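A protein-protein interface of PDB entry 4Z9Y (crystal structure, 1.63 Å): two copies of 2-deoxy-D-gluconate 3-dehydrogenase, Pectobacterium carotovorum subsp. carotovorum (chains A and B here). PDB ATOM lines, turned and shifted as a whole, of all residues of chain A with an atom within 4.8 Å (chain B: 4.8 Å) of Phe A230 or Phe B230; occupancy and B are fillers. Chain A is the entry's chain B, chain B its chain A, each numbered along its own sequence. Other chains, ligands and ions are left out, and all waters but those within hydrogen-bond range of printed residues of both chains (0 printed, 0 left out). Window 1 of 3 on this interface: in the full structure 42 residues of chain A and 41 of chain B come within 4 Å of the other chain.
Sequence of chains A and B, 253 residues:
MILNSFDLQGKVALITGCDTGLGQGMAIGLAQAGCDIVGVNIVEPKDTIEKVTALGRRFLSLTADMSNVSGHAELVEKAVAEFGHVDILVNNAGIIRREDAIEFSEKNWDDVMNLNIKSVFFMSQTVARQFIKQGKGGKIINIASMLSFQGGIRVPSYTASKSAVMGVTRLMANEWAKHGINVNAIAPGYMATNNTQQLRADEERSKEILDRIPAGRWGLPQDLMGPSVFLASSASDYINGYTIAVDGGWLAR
The backbone carbonyl oxygen of Val A229 sits close to the side-chain hydroxyl of Ser A233, 3.5 Å away.
O of Val B229 sits close to OG of Ser B233, 3.4 Å away.
The side-chain hydroxyl of Ser B233 sits close to the backbone NH of Ala B235, at 3.1 Å.
The side-chain hydroxyl of Ser A233 is in hydrogen-bond range of the backbone carbonyl oxygen of Phe A230 (2.9 Å).
The backbone carbonyl oxygen (O) of Phe A230 sits at hydrogen-bond distance from the side-chain hydroxyl (OG) of Ser A236.
OG of Ser B236 sits at hydrogen-bond distance from O of Phe B230, at 2.8 Å.
Among the printed residues, pairs that only touch across the chains: Ala A235 with Pro B227 (3.3 Å), Pro A227 with Ala B235 (3.3 Å), Phe A6 with Phe B6 (3.4 Å), Ala A235 with Gly B226 (3.4 Å), Gly A226 with Ala B235 (3.5 Å), Phe A230 with Phe B230 (3.5 Å), Phe A6 with Gly B226 (3.6 Å), Gly A226 with Phe B6 (3.7 Å), Pro A227 with Phe B230 (3.7 Å), Phe A230 with Pro B227 (3.8 Å), Val A229 with Phe B6 (3.8 Å), Phe A230 with Gly B226 (3.8 Å), Gly A226 with Phe B230 (3.8 Å), Ile A244 with Ile B239 (3.8 Å), Ile A239 with Ile B244 (3.9 Å), Phe A6 with Val B229 (3.9 Å) and Ile A244 with Ile B244 (3.97 Å).
Of chain B, only Gly B226 (3.8 Å), Pro B227 (3.8 Å) and Phe B230 (3.5 Å) come within 4 Å of Phe A230.
Of the printed residues of chain A, Phe B6 touches Phe A6 (3.4 Å), Gly A226 (3.7 Å) and Val A229 (3.8 Å).
Of the printed residues of chain A, Val B229 touches Phe A6 (3.9 Å).
Phe B230 touches just these residues of chain A: Gly A226 (3.8 Å), Pro A227 (3.7 Å) and Phe A230 (3.5 Å).
Of the printed residues of chain A, Ala B235 touches Gly A226 (3.5 Å) and Pro A227 (3.3 Å).
Of the printed residues of chain A, Ile B239 touches Ile A244 (3.8 Å).
Printed residues of chain A within 4 Å of Ile B244: Ile A239 and Ile A244.
The nearest residue of chain A that does not touch Phe B230 is Phe A6 (4.3 Å).
The nearest printed residue of chain A that does not touch Ala B235 is Phe A230 (6.5 Å).
Printed residues of chain B that touch a printed residue of chain A: Phe B6, Gly B226, Pro B227, Val B229, Phe B230, Ala B235, Ile B239 and Ile B244.
Among the printed residues, 17 pairs touch across the chains.
Among the printed residues, no Asp or Glu carboxylate lies within 4 Å of a Lys or Arg side-chain nitrogen of the other chain.
Phe A6 touches Gly B226, and with the chains exchanged Gly A226 touches Phe B6.
Gly A226 touches Ala B235, and with the chains exchanged Ala A235 touches Gly B226.
Pro A227 touches Phe B230, and with the chains exchanged Phe A230 touches Pro B227.
Phe A230 touches its own counterpart, Phe B230.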
ATOM      1  N   PHE A   6      11.234 -28.913 -25.292  1.00  0.00           N
ATOM      2  CA  PHE A   6       9.860 -29.113 -24.792  1.00  0.00           C
ATOM      3  C   PHE A   6       9.246 -30.425 -25.301  1.00  0.00           C
ATOM      4  O   PHE A   6       8.209 -30.860 -24.802  1.00  0.00           O
ATOM      5  CB  PHE A   6       8.944 -27.966 -25.225  1.00  0.00           C
ATOM      6  CG  PHE A   6       9.341 -26.613 -24.691  1.00  0.00           C
ATOM      7  CD1 PHE A   6       8.927 -26.201 -23.444  1.00  0.00           C
ATOM      8  CD2 PHE A   6      10.089 -25.740 -25.460  1.00  0.00           C
ATOM      9  CE1 PHE A   6       9.262 -24.949 -22.961  1.00  0.00           C
ATOM     10  CE2 PHE A   6      10.434 -24.479 -24.977  1.00  0.00           C
ATOM     11  CZ  PHE A   6      10.022 -24.096 -23.727  1.00  0.00           C
ATOM     12  N   GLY A 226       0.454 -26.565 -20.793  1.00  0.00           N
ATOM     13  CA  GLY A 226       1.759 -25.963 -21.015  1.00  0.00           C
ATOM     14  C   GLY A 226       2.674 -26.051 -19.818  1.00  0.00           C
ATOM     15  O   GLY A 226       3.815 -26.480 -19.944  1.00  0.00           O
ATOM     16  N   PRO A 227       2.180 -25.652 -18.642  1.00  0.00           N
ATOM     17  CA  PRO A 227       3.041 -25.703 -17.463  1.00  0.00           C
ATOM     18  C   PRO A 227       3.505 -27.120 -17.095  1.00  0.00           C
ATOM     19  O   PRO A 227       4.648 -27.295 -16.669  1.00  0.00           O
ATOM     20  CB  PRO A 227       2.169 -25.084 -16.371  1.00  0.00           C
ATOM     21  CG  PRO A 227       1.262 -24.160 -17.125  1.00  0.00           C
ATOM     22  CD  PRO A 227       0.943 -24.890 -18.383  1.00  0.00           C
ATOM     23  N   SER A 228       2.627 -28.109 -17.255  1.00  0.00           N
ATOM     24  CA  SER A 228       2.993 -29.481 -16.947  1.00  0.00           C
ATOM     25  C   SER A 228       4.017 -30.003 -17.973  1.00  0.00           C
ATOM     26  O   SER A 228       5.005 -30.628 -17.601  1.00  0.00           O
ATOM     27  CB  SER A 228       1.735 -30.376 -16.807  1.00  0.00           C
ATOM     28  OG  SER A 228       1.084 -30.588 -18.030  1.00  0.00           O
ATOM     29  N   VAL A 229       3.818 -29.736 -19.255  1.00  0.00           N
ATOM     30  CA  VAL A 229       4.803 -30.160 -20.255  1.00  0.00           C
ATOM     31  C   VAL A 229       6.160 -29.501 -19.973  1.00  0.00           C
ATOM     32  O   VAL A 229       7.193 -30.156 -19.984  1.00  0.00           O
ATOM     33  CB  VAL A 229       4.299 -29.840 -21.680  1.00  0.00           C
ATOM     34  CG1 VAL A 229       5.432 -29.929 -22.714  1.00  0.00           C
ATOM     35  CG2 VAL A 229       3.153 -30.769 -22.043  1.00  0.00           C
ATOM     36  N   PHE A 230       6.145 -28.196 -19.713  1.00  0.00           N
ATOM     37  CA  PHE A 230       7.350 -27.449 -19.336  1.00  0.00           C
ATOM     38  C   PHE A 230       8.129 -28.117 -18.184  1.00  0.00           C
ATOM     39  O   PHE A 230       9.322 -28.404 -18.316  1.00  0.00           O
ATOM     40  CB  PHE A 230       6.935 -26.019 -18.974  1.00  0.00           C
ATOM     41  CG  PHE A 230       8.041 -25.172 -18.407  1.00  0.00           C
ATOM     42  CD1 PHE A 230       9.162 -24.858 -19.157  1.00  0.00           C
ATOM     43  CD2 PHE A 230       7.927 -24.646 -17.127  1.00  0.00           C
ATOM     44  CE1 PHE A 230      10.157 -24.044 -18.632  1.00  0.00           C
ATOM     45  CE2 PHE A 230       8.907 -23.827 -16.600  1.00  0.00           C
ATOM     46  CZ  PHE A 230      10.026 -23.528 -17.362  1.00  0.00           C
ATOM     47  N   LEU A 231       7.443 -28.387 -17.081  1.00  0.00           N
ATOM     48  CA  LEU A 231       8.067 -28.980 -15.897  1.00  0.00           C
ATOM     49  C   LEU A 231       8.427 -30.456 -16.092  1.00  0.00           C
ATOM     50  O   LEU A 231       9.214 -30.994 -15.330  1.00  0.00           O
ATOM     51  CB  LEU A 231       7.161 -28.820 -14.659  1.00  0.00           C
ATOM     52  CG  LEU A 231       7.024 -27.393 -14.126  1.00  0.00           C
ATOM     53  CD1 LEU A 231       6.010 -27.392 -12.991  1.00  0.00           C
ATOM     54  CD2 LEU A 231       8.363 -26.818 -13.652  1.00  0.00           C
ATOM     55  N   ALA A 232       7.855 -31.100 -17.107  1.00  0.00           N
ATOM     56  CA  ALA A 232       8.178 -32.494 -17.447  1.00  0.00           C
ATOM     57  C   ALA A 232       9.309 -32.612 -18.464  1.00  0.00           C
ATOM     58  O   ALA A 232       9.706 -33.727 -18.832  1.00  0.00           O
ATOM     59  CB  ALA A 232       6.940 -33.189 -17.995  1.00  0.00           C
ATOM     60  N   SER A 233       9.837 -31.476 -18.919  1.00  0.00           N
ATOM     61  CA  SER A 233      10.778 -31.430 -20.037  1.00  0.00           C
ATOM     62  C   SER A 233      12.150 -30.871 -19.656  1.00  0.00           C
ATOM     63  O   SER A 233      12.338 -30.279 -18.594  1.00  0.00           O
ATOM     64  CB  SER A 233      10.212 -30.549 -21.153  1.00  0.00           C
ATOM     65  OG  SER A 233      10.389 -29.171 -20.859  1.00  0.00           O
ATOM     66  N   ALA A 235      13.374 -28.318 -20.841  1.00  0.00           N
ATOM     67  CA  ALA A 235      13.294 -26.868 -20.839  1.00  0.00           C
ATOM     68  C   ALA A 235      13.282 -26.265 -19.443  1.00  0.00           C
ATOM     69  O   ALA A 235      13.447 -25.052 -19.305  1.00  0.00           O
ATOM     70  CB  ALA A 235      12.065 -26.422 -21.612  1.00  0.00           C
ATOM     71  N   SER A 236      13.073 -27.082 -18.412  1.00  0.00           N
ATOM     72  CA  SER A 236      13.055 -26.609 -17.036  1.00  0.00           C
ATOM     73  C   SER A 236      14.101 -27.294 -16.160  1.00  0.00           C
ATOM     74  O   SER A 236      13.903 -27.396 -14.959  1.00  0.00           O
ATOM     75  CB  SER A 236      11.656 -26.807 -16.446  1.00  0.00           C
ATOM     76  OG  SER A 236      11.283 -28.175 -16.435  1.00  0.00           O
ATOM     77  N   ILE A 239      15.111 -25.737 -12.832  1.00  0.00           N
ATOM     78  CA  ILE A 239      14.049 -25.433 -11.875  1.00  0.00           C
ATOM     79  C   ILE A 239      13.896 -26.652 -10.998  1.00  0.00           C
ATOM     80  O   ILE A 239      13.709 -27.762 -11.510  1.00  0.00           O
ATOM     81  CB  ILE A 239      12.724 -25.119 -12.587  1.00  0.00           C
ATOM     82  CG1 ILE A 239      12.932 -23.911 -13.517  1.00  0.00           C
ATOM     83  CG2 ILE A 239      11.599 -24.862 -11.582  1.00  0.00           C
ATOM     84  CD1 ILE A 239      11.688 -23.472 -14.237  1.00  0.00           C
ATOM     85  N   ILE A 244       5.068 -23.391  -8.888  1.00  0.00           N
ATOM     86  CA  ILE A 244       4.626 -22.380  -9.844  1.00  0.00           C
ATOM     87  C   ILE A 244       3.108 -22.241  -9.784  1.00  0.00           C
ATOM     88  O   ILE A 244       2.382 -23.203 -10.015  1.00  0.00           O
ATOM     89  CB  ILE A 244       5.032 -22.764 -11.272  1.00  0.00           C
ATOM     90  CG1 ILE A 244       6.553 -22.895 -11.366  1.00  0.00           C
ATOM     91  CG2 ILE A 244       4.512 -21.720 -12.254  1.00  0.00           C
ATOM     92  CD1 ILE A 244       7.061 -23.378 -12.703  1.00  0.00           C
ATOM     93  N   PHE B   6       4.274 -23.277 -27.526  1.00  0.00           N
ATOM     94  CA  PHE B   6       5.604 -22.771 -27.181  1.00  0.00           C
ATOM     95  C   PHE B   6       6.267 -22.058 -28.348  1.00  0.00           C
ATOM     96  O   PHE B   6       7.287 -21.395 -28.172  1.00  0.00           O
ATOM     97  CB  PHE B   6       6.529 -23.917 -26.766  1.00  0.00           C
ATOM     98  CG  PHE B   6       6.059 -24.682 -25.567  1.00  0.00           C
ATOM     99  CD1 PHE B   6       6.191 -24.168 -24.292  1.00  0.00           C
ATOM    100  CD2 PHE B   6       5.522 -25.947 -25.711  1.00  0.00           C
ATOM    101  CE1 PHE B   6       5.764 -24.897 -23.182  1.00  0.00           C
ATOM    102  CE2 PHE B   6       5.086 -26.669 -24.607  1.00  0.00           C
ATOM    103  CZ  PHE B   6       5.202 -26.143 -23.346  1.00  0.00           C
ATOM    104  N   GLY B 226      14.701 -22.015 -21.899  1.00  0.00           N
ATOM    105  CA  GLY B 226      13.393 -22.645 -21.759  1.00  0.00           C
ATOM    106  C   GLY B 226      12.409 -21.850 -20.923  1.00  0.00           C
ATOM    107  O   GLY B 226      11.271 -21.638 -21.338  1.00  0.00           O
ATOM    108  N   PRO B 227      12.816 -21.421 -19.721  1.00  0.00           N
ATOM    109  CA  PRO B 227      11.895 -20.646 -18.877  1.00  0.00           C
ATOM    110  C   PRO B 227      11.466 -19.342 -19.518  1.00  0.00           C
ATOM    111  O   PRO B 227      10.296 -18.957 -19.395  1.00  0.00           O
ATOM    112  CB  PRO B 227      12.698 -20.428 -17.593  1.00  0.00           C
ATOM    113  CG  PRO B 227      13.579 -21.636 -17.532  1.00  0.00           C
ATOM    114  CD  PRO B 227      14.000 -21.865 -18.962  1.00  0.00           C
ATOM    115  N   SER B 228      12.372 -18.672 -20.231  1.00  0.00           N
ATOM    116  CA  SER B 228      11.995 -17.423 -20.868  1.00  0.00           C
ATOM    117  C   SER B 228      11.058 -17.656 -22.068  1.00  0.00           C
ATOM    118  O   SER B 228      10.079 -16.943 -22.219  1.00  0.00           O
ATOM    119  CB  SER B 228      13.222 -16.567 -21.229  1.00  0.00           C
ATOM    120  OG  SER B 228      13.959 -17.134 -22.280  1.00  0.00           O
ATOM    121  N   VAL B 229      11.320 -18.674 -22.896  1.00  0.00           N
ATOM    122  CA  VAL B 229      10.376 -19.016 -23.978  1.00  0.00           C
ATOM    123  C   VAL B 229       8.995 -19.370 -23.402  1.00  0.00           C
ATOM    124  O   VAL B 229       7.962 -18.928 -23.888  1.00  0.00           O
ATOM    125  CB  VAL B 229      10.941 -20.167 -24.837  1.00  0.00           C
ATOM    126  CG1 VAL B 229       9.897 -20.722 -25.797  1.00  0.00           C
ATOM    127  CG2 VAL B 229      12.145 -19.658 -25.619  1.00  0.00           C
ATOM    128  N   PHE B 230       8.992 -20.167 -22.346  1.00  0.00           N
ATOM    129  CA  PHE B 230       7.756 -20.573 -21.700  1.00  0.00           C
ATOM    130  C   PHE B 230       6.927 -19.371 -21.279  1.00  0.00           C
ATOM    131  O   PHE B 230       5.746 -19.266 -21.630  1.00  0.00           O
ATOM    132  CB  PHE B 230       8.104 -21.452 -20.494  1.00  0.00           C
ATOM    133  CG  PHE B 230       6.945 -21.790 -19.604  1.00  0.00           C
ATOM    134  CD1 PHE B 230       5.877 -22.535 -20.066  1.00  0.00           C
ATOM    135  CD2 PHE B 230       6.954 -21.403 -18.272  1.00  0.00           C
ATOM    136  CE1 PHE B 230       4.831 -22.865 -19.226  1.00  0.00           C
ATOM    137  CE2 PHE B 230       5.916 -21.732 -17.412  1.00  0.00           C
ATOM    138  CZ  PHE B 230       4.850 -22.466 -17.887  1.00  0.00           C
ATOM    139  N   LEU B 231       7.551 -18.458 -20.538  1.00  0.00           N
ATOM    140  CA  LEU B 231       6.856 -17.270 -20.050  1.00  0.00           C
ATOM    141  C   LEU B 231       6.516 -16.263 -21.145  1.00  0.00           C
ATOM    142  O   LEU B 231       5.639 -15.423 -20.962  1.00  0.00           O
ATOM    143  CB  LEU B 231       7.686 -16.599 -18.948  1.00  0.00           C
ATOM    144  CG  LEU B 231       7.716 -17.371 -17.626  1.00  0.00           C
ATOM    145  CD1 LEU B 231       8.653 -16.665 -16.662  1.00  0.00           C
ATOM    146  CD2 LEU B 231       6.323 -17.504 -17.013  1.00  0.00           C
ATOM    147  N   ALA B 232       7.198 -16.360 -22.281  1.00  0.00           N
ATOM    148  CA  ALA B 232       6.926 -15.508 -23.441  1.00  0.00           C
ATOM    149  C   ALA B 232       5.856 -16.071 -24.374  1.00  0.00           C
ATOM    150  O   ALA B 232       5.527 -15.451 -25.398  1.00  0.00           O
ATOM    151  CB  ALA B 232       8.210 -15.287 -24.220  1.00  0.00           C
ATOM    152  N   SER B 233       5.332 -17.256 -24.047  1.00  0.00           N
ATOM    153  CA  SER B 233       4.474 -18.028 -24.955  1.00  0.00           C
ATOM    154  C   SER B 233       3.061 -18.226 -24.422  1.00  0.00           C
ATOM    155  O   SER B 233       2.782 -18.006 -23.240  1.00  0.00           O
ATOM    156  CB  SER B 233       5.096 -19.395 -25.226  1.00  0.00           C
ATOM    157  OG  SER B 233       4.847 -20.292 -24.158  1.00  0.00           O
ATOM    158  N   ALA B 235       1.796 -20.918 -23.831  1.00  0.00           N
ATOM    159  CA  ALA B 235       1.835 -22.069 -22.916  1.00  0.00           C
ATOM    160  C   ALA B 235       1.742 -21.655 -21.450  1.00  0.00           C
ATOM    161  O   ALA B 235       1.532 -22.503 -20.578  1.00  0.00           O
ATOM    162  CB  ALA B 235       3.098 -22.894 -23.151  1.00  0.00           C
ATOM    163  N   SER B 236       1.912 -20.365 -21.158  1.00  0.00           N
ATOM    164  CA  SER B 236       1.856 -19.874 -19.784  1.00  0.00           C
ATOM    165  C   SER B 236       0.776 -18.815 -19.585  1.00  0.00           C
ATOM    166  O   SER B 236       0.890 -17.968 -18.700  1.00  0.00           O
ATOM    167  CB  SER B 236       3.221 -19.318 -19.367  1.00  0.00           C
ATOM    168  OG  SER B 236       3.621 -18.251 -20.199  1.00  0.00           O
ATOM    169  N   ILE B 239      -0.515 -18.000 -16.092  1.00  0.00           N
ATOM    170  CA  ILE B 239       0.492 -17.607 -15.125  1.00  0.00           C
ATOM    171  C   ILE B 239       0.610 -16.090 -15.204  1.00  0.00           C
ATOM    172  O   ILE B 239       0.880 -15.531 -16.270  1.00  0.00           O
ATOM    173  CB  ILE B 239       1.858 -18.276 -15.398  1.00  0.00           C
ATOM    174  CG1 ILE B 239       1.704 -19.802 -15.337  1.00  0.00           C
ATOM    175  CG2 ILE B 239       2.898 -17.799 -14.378  1.00  0.00           C
ATOM    176  CD1 ILE B 239       2.979 -20.566 -15.590  1.00  0.00           C
ATOM    177  N   ILE B 244       9.219 -17.085 -10.919  1.00  0.00           N
ATOM    178  CA  ILE B 244       9.687 -18.480 -11.005  1.00  0.00           C
ATOM    179  C   ILE B 244      11.192 -18.522 -10.796  1.00  0.00           C
ATOM    180  O   ILE B 244      11.952 -17.898 -11.553  1.00  0.00           O
ATOM    181  CB  ILE B 244       9.362 -19.116 -12.367  1.00  0.00           C
ATOM    182  CG1 ILE B 244       7.852 -19.135 -12.595  1.00  0.00           C
ATOM    183  CG2 ILE B 244       9.893 -20.547 -12.425  1.00  0.00           C
ATOM    184  CD1 ILE B 244       7.444 -19.633 -13.961  1.00  0.00           C
